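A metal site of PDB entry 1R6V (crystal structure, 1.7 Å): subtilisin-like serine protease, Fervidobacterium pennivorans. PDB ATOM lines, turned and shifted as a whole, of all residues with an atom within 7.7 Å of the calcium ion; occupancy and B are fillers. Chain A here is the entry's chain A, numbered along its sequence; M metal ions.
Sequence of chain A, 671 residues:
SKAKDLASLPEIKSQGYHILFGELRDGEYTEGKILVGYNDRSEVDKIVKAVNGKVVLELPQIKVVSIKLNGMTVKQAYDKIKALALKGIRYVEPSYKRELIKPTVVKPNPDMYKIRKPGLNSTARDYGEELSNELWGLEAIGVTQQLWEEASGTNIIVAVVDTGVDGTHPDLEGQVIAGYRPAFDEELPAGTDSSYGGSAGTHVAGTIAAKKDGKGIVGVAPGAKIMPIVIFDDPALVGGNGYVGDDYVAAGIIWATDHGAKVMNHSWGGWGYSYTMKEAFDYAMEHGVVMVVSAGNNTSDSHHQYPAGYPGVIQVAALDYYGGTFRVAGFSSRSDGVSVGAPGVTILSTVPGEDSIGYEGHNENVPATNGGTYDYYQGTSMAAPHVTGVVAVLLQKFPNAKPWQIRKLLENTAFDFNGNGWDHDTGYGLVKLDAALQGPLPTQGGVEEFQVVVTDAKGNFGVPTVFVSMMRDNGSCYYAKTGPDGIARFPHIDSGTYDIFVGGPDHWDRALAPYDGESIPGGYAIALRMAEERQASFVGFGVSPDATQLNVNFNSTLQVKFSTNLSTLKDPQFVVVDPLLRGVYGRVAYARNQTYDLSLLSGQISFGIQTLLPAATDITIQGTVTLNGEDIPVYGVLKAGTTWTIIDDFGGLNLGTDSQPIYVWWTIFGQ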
ATOM      1  N   GLY A 128     -21.352   9.350 -14.289  1.00  0.00           N
ATOM      2  CA  GLY A 128     -20.542   8.380 -15.018  1.00  0.00           C
ATOM      3  C   GLY A 128     -19.244   7.926 -14.377  1.00  0.00           C
ATOM      4  O   GLY A 128     -18.626   6.958 -14.823  1.00  0.00           O
ATOM      5  N   GLU A 129     -18.827   8.619 -13.317  1.00  0.00           N
ATOM      6  CA  GLU A 129     -17.579   8.303 -12.623  1.00  0.00           C
ATOM      7  C   GLU A 129     -17.862   7.464 -11.384  1.00  0.00           C
ATOM      8  O   GLU A 129     -18.902   7.622 -10.758  1.00  0.00           O
ATOM      9  CB  GLU A 129     -16.892   9.594 -12.174  1.00  0.00           C
ATOM     10  CG  GLU A 129     -16.897  10.669 -13.242  1.00  0.00           C
ATOM     11  CD  GLU A 129     -16.102  10.283 -14.452  1.00  0.00           C
ATOM     12  OE1 GLU A 129     -14.879  10.524 -14.431  1.00  0.00           O
ATOM     13  OE2 GLU A 129     -16.691   9.745 -15.417  1.00  0.00           O
ATOM     14  N   GLU A 130     -16.906   6.625 -11.014  1.00  0.00           N
ATOM     15  CA  GLU A 130     -17.081   5.764  -9.856  1.00  0.00           C
ATOM     16  C   GLU A 130     -17.341   6.521  -8.557  1.00  0.00           C
ATOM     17  O   GLU A 130     -17.993   5.990  -7.663  1.00  0.00           O
ATOM     18  CB  GLU A 130     -15.875   4.846  -9.697  1.00  0.00           C
ATOM     19  CG  GLU A 130     -14.613   5.588  -9.355  1.00  0.00           C
ATOM     20  CD  GLU A 130     -13.368   4.756  -9.616  1.00  0.00           C
ATOM     21  OE1 GLU A 130     -12.266   5.312  -9.501  1.00  0.00           O
ATOM     22  OE2 GLU A 130     -13.497   3.546  -9.931  1.00  0.00           O
ATOM     23  N   LEU A 131     -16.859   7.758  -8.451  1.00  0.00           N
ATOM     24  CA  LEU A 131     -17.089   8.533  -7.226  1.00  0.00           C
ATOM     25  C   LEU A 131     -18.225   9.547  -7.332  1.00  0.00           C
ATOM     26  O   LEU A 131     -18.391  10.379  -6.449  1.00  0.00           O
ATOM     27  CB  LEU A 131     -15.791   9.234  -6.793  1.00  0.00           C
ATOM     28  CG  LEU A 131     -14.585   8.298  -6.600  1.00  0.00           C
ATOM     29  CD1 LEU A 131     -13.361   9.105  -6.185  1.00  0.00           C
ATOM     30  CD2 LEU A 131     -14.914   7.217  -5.562  1.00  0.00           C
ATOM     31  N   PRO A 170      -3.794  11.007 -12.306  1.00  0.00           N
ATOM     32  CA  PRO A 170      -4.505  10.311 -13.380  1.00  0.00           C
ATOM     33  C   PRO A 170      -5.814  10.986 -13.787  1.00  0.00           C
ATOM     34  O   PRO A 170      -6.136  11.025 -14.980  1.00  0.00           O
ATOM     35  CB  PRO A 170      -4.681   8.895 -12.830  1.00  0.00           C
ATOM     36  CG  PRO A 170      -4.659   9.080 -11.338  1.00  0.00           C
ATOM     37  CD  PRO A 170      -3.596  10.133 -11.139  1.00  0.00           C
ATOM     38  N   ASP A 171      -6.545  11.550 -12.829  1.00  0.00           N
ATOM     39  CA  ASP A 171      -7.810  12.232 -13.125  1.00  0.00           C
ATOM     40  C   ASP A 171      -7.594  13.581 -13.831  1.00  0.00           C
ATOM     41  O   ASP A 171      -8.563  14.270 -14.161  1.00  0.00           O
ATOM     42  CB  ASP A 171      -8.599  12.475 -11.821  1.00  0.00           C
ATOM     43  CG  ASP A 171     -10.034  11.957 -11.880  1.00  0.00           C
ATOM     44  OD1 ASP A 171     -10.550  11.699 -12.985  1.00  0.00           O
ATOM     45  OD2 ASP A 171     -10.644  11.824 -10.804  1.00  0.00           O
ATOM     46  N   LEU A 172      -6.344  13.988 -14.024  1.00  0.00           N
ATOM     47  CA  LEU A 172      -6.070  15.246 -14.702  1.00  0.00           C
ATOM     48  C   LEU A 172      -5.323  15.015 -16.007  1.00  0.00           C
ATOM     49  O   LEU A 172      -4.873  15.964 -16.647  1.00  0.00           O
ATOM     50  CB  LEU A 172      -5.258  16.198 -13.814  1.00  0.00           C
ATOM     51  CG  LEU A 172      -5.971  16.669 -12.538  1.00  0.00           C
ATOM     52  CD1 LEU A 172      -5.039  17.581 -11.726  1.00  0.00           C
ATOM     53  CD2 LEU A 172      -7.240  17.449 -12.921  1.00  0.00           C
ATOM     54  N   ALA A 209     -12.016  20.836 -13.645  1.00  0.00           N
ATOM     55  CA  ALA A 209     -11.916  19.995 -14.829  1.00  0.00           C
ATOM     56  C   ALA A 209     -11.385  18.569 -14.689  1.00  0.00           C
ATOM     57  O   ALA A 209     -10.703  18.081 -15.586  1.00  0.00           O
ATOM     58  CB  ALA A 209     -11.073  20.731 -15.873  1.00  0.00           C
ATOM     59  N   ALA A 210     -11.671  17.877 -13.588  1.00  0.00           N
ATOM     60  CA  ALA A 210     -11.196  16.506 -13.511  1.00  0.00           C
ATOM     61  C   ALA A 210     -11.801  15.790 -14.727  1.00  0.00           C
ATOM     62  O   ALA A 210     -12.951  16.013 -15.110  1.00  0.00           O
ATOM     63  CB  ALA A 210     -11.635  15.839 -12.206  1.00  0.00           C
ATOM     64  N   LYS A 211     -11.004  14.919 -15.342  1.00  0.00           N
ATOM     65  CA  LYS A 211     -11.418  14.195 -16.544  1.00  0.00           C
ATOM     66  C   LYS A 211     -12.643  13.291 -16.438  1.00  0.00           C
ATOM     67  O   LYS A 211     -12.784  12.551 -15.476  1.00  0.00           O
ATOM     68  CB  LYS A 211     -10.216  13.375 -17.026  1.00  0.00           C
ATOM     69  CG  LYS A 211     -10.324  12.740 -18.389  1.00  0.00           C
ATOM     70  CD  LYS A 211      -9.115  11.824 -18.610  1.00  0.00           C
ATOM     71  CE  LYS A 211      -9.127  11.174 -19.992  1.00  0.00           C
ATOM     72  NZ  LYS A 211      -7.994  10.227 -20.174  1.00  0.00           N
ATOM     73  N   LYS A 212     -13.538  13.360 -17.417  1.00  0.00           N
ATOM     74  CA  LYS A 212     -14.707  12.481 -17.403  1.00  0.00           C
ATOM     75  C   LYS A 212     -14.197  11.193 -18.063  1.00  0.00           C
ATOM     76  O   LYS A 212     -14.067  11.126 -19.286  1.00  0.00           O
ATOM     77  CB  LYS A 212     -15.843  13.086 -18.215  1.00  0.00           C
ATOM     78  CG  LYS A 212     -17.159  12.371 -18.040  1.00  0.00           C
ATOM     79  CD  LYS A 212     -18.259  13.147 -18.735  1.00  0.00           C
ATOM     80  CE  LYS A 212     -19.610  12.492 -18.540  1.00  0.00           C
ATOM     81  NZ  LYS A 212     -19.637  11.063 -18.993  1.00  0.00           N
ATOM     82  N   ASP A 213     -13.896  10.190 -17.258  1.00  0.00           N
ATOM     83  CA  ASP A 213     -13.356   8.944 -17.798  1.00  0.00           C
ATOM     84  C   ASP A 213     -13.797   7.709 -17.032  1.00  0.00           C
ATOM     85  O   ASP A 213     -13.160   6.655 -17.124  1.00  0.00           O
ATOM     86  CB  ASP A 213     -11.819   9.016 -17.785  1.00  0.00           C
ATOM     87  CG  ASP A 213     -11.260   9.179 -16.388  1.00  0.00           C
ATOM     88  OD1 ASP A 213     -12.055   9.294 -15.444  1.00  0.00           O
ATOM     89  OD2 ASP A 213     -10.011   9.182 -16.230  1.00  0.00           O
ATOM     90  N   GLY A 214     -14.887   7.844 -16.271  1.00  0.00           N
ATOM     91  CA  GLY A 214     -15.413   6.733 -15.498  1.00  0.00           C
ATOM     92  C   GLY A 214     -14.731   6.486 -14.167  1.00  0.00           C
ATOM     93  O   GLY A 214     -15.290   5.797 -13.301  1.00  0.00           O
ATOM     94  N   LYS A 215     -13.546   7.048 -13.992  1.00  0.00           N
ATOM     95  CA  LYS A 215     -12.768   6.861 -12.757  1.00  0.00           C
ATOM     96  C   LYS A 215     -12.694   8.129 -11.914  1.00  0.00           C
ATOM     97  O   LYS A 215     -12.873   9.226 -12.412  1.00  0.00           O
ATOM     98  CB  LYS A 215     -11.343   6.455 -13.125  1.00  0.00           C
ATOM     99  CG  LYS A 215     -11.247   5.236 -14.045  1.00  0.00           C
ATOM    100  CD  LYS A 215     -11.551   3.958 -13.263  1.00  0.00           C
ATOM    101  CE  LYS A 215     -11.251   2.708 -14.086  1.00  0.00           C
ATOM    102  NZ  LYS A 215     -11.380   1.484 -13.253  1.00  0.00           N
ATOM    103  N   GLY A 216     -12.423   7.965 -10.625  1.00  0.00           N
ATOM    104  CA  GLY A 216     -12.306   9.109  -9.720  1.00  0.00           C
ATOM    105  C   GLY A 216     -13.494  10.056  -9.776  1.00  0.00           C
ATOM    106  O   GLY A 216     -14.638   9.614  -9.739  1.00  0.00           O
ATOM    107  N   ILE A 217     -13.232  11.358  -9.848  1.00  0.00           N
ATOM    108  CA  ILE A 217     -14.308  12.344  -9.905  1.00  0.00           C
ATOM    109  C   ILE A 217     -14.360  12.977 -11.298  1.00  0.00           C
ATOM    110  O   ILE A 217     -13.700  12.503 -12.228  1.00  0.00           O
ATOM    111  CB  ILE A 217     -14.115  13.471  -8.844  1.00  0.00           C
ATOM    112  CG1 ILE A 217     -12.843  14.280  -9.121  1.00  0.00           C
ATOM    113  CG2 ILE A 217     -13.968  12.838  -7.454  1.00  0.00           C
ATOM    114  CD1 ILE A 217     -12.942  15.740  -8.642  1.00  0.00           C
ATOM    115  N   VAL A 218     -15.167  14.014 -11.452  1.00  0.00           N
ATOM    116  CA  VAL A 218     -15.235  14.698 -12.740  1.00  0.00           C
ATOM    117  C   VAL A 218     -15.462  16.164 -12.383  1.00  0.00           C
ATOM    118  O   VAL A 218     -16.090  16.467 -11.359  1.00  0.00           O
ATOM    119  CB  VAL A 218     -16.374  14.137 -13.638  1.00  0.00           C
ATOM    120  CG1 VAL A 218     -17.714  14.206 -12.921  1.00  0.00           C
ATOM    121  CG2 VAL A 218     -16.424  14.903 -14.981  1.00  0.00           C
ATOM    122  N   GLY A 219     -14.908  17.068 -13.169  1.00  0.00           N
ATOM    123  CA  GLY A 219     -15.050  18.485 -12.896  1.00  0.00           C
ATOM    124  C   GLY A 219     -16.366  19.057 -13.387  1.00  0.00           C
ATOM    125  O   GLY A 219     -17.131  18.379 -14.064  1.00  0.00           O
ATOM    126  N   THR A 350      -9.203  15.983  -6.385  1.00  0.00           N
ATOM    127  CA  THR A 350      -7.840  15.515  -6.578  1.00  0.00           C
ATOM    128  C   THR A 350      -6.803  16.247  -5.712  1.00  0.00           C
ATOM    129  O   THR A 350      -6.885  17.462  -5.541  1.00  0.00           O
ATOM    130  CB  THR A 350      -7.441  15.712  -8.063  1.00  0.00           C
ATOM    131  OG1 THR A 350      -7.811  17.033  -8.484  1.00  0.00           O
ATOM    132  CG2 THR A 350      -8.161  14.719  -8.957  1.00  0.00           C
ATOM    133  N   ASN A 370      -8.122   4.256  -9.905  1.00  0.00           N
ATOM    134  CA  ASN A 370      -7.155   4.742 -10.878  1.00  0.00           C
ATOM    135  C   ASN A 370      -5.790   5.025 -10.261  1.00  0.00           C
ATOM    136  O   ASN A 370      -4.908   5.564 -10.922  1.00  0.00           O
ATOM    137  CB  ASN A 370      -7.682   6.013 -11.553  1.00  0.00           C
ATOM    138  CG  ASN A 370      -8.035   7.086 -10.565  1.00  0.00           C
ATOM    139  OD1 ASN A 370      -7.820   6.938  -9.357  1.00  0.00           O
ATOM    140  ND2 ASN A 370      -8.582   8.198 -11.060  1.00  0.00           N
ATOM    141  N   TYR A 374      -7.091  11.458  -3.344  1.00  0.00           N
ATOM    142  CA  TYR A 374      -8.183  12.420  -3.217  1.00  0.00           C
ATOM    143  C   TYR A 374      -8.367  12.805  -1.767  1.00  0.00           C
ATOM    144  O   TYR A 374      -7.912  12.111  -0.877  1.00  0.00           O
ATOM    145  CB  TYR A 374      -9.499  11.798  -3.677  1.00  0.00           C
ATOM    146  CG  TYR A 374      -9.486  11.376  -5.120  1.00  0.00           C
ATOM    147  CD1 TYR A 374      -8.879  10.187  -5.525  1.00  0.00           C
ATOM    148  CD2 TYR A 374     -10.041  12.207  -6.106  1.00  0.00           C
ATOM    149  CE1 TYR A 374      -8.809   9.836  -6.862  1.00  0.00           C
ATOM    150  CE2 TYR A 374      -9.977  11.875  -7.435  1.00  0.00           C
ATOM    151  CZ  TYR A 374      -9.353  10.694  -7.817  1.00  0.00           C
ATOM    152  OH  TYR A 374      -9.263  10.399  -9.154  1.00  0.00           O
HETATM  153 CA    CA M   1     -12.667  11.066 -13.750  1.00  0.00          CA
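OD2 of Asp 171 is in hydrogen-bond range of OH of Tyr 374 (2.6 Å).
The side-chain carboxylate of Glu 129 lies within hydrogen-bond range of the backbone NH of Gly 214 (2.8 Å).
O of Lys 211 is bound to the calcium ion (2.3 Å).
The backbone carbonyl oxygen (O) of Lys 215 is bound to the calcium ion (2.3 Å).
O of Ile 217 is bound to the calcium ion, at 2.3 Å.
The calcium ion is bound by the side-chain carboxylate (OD1) of Asp 171.
The calcium ion is bound by OE1 of Glu 129 (2.4 Å).
The side-chain carboxylate (OD1) of Asp 213 is bound to the calcium ion, 2.5 Å away.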
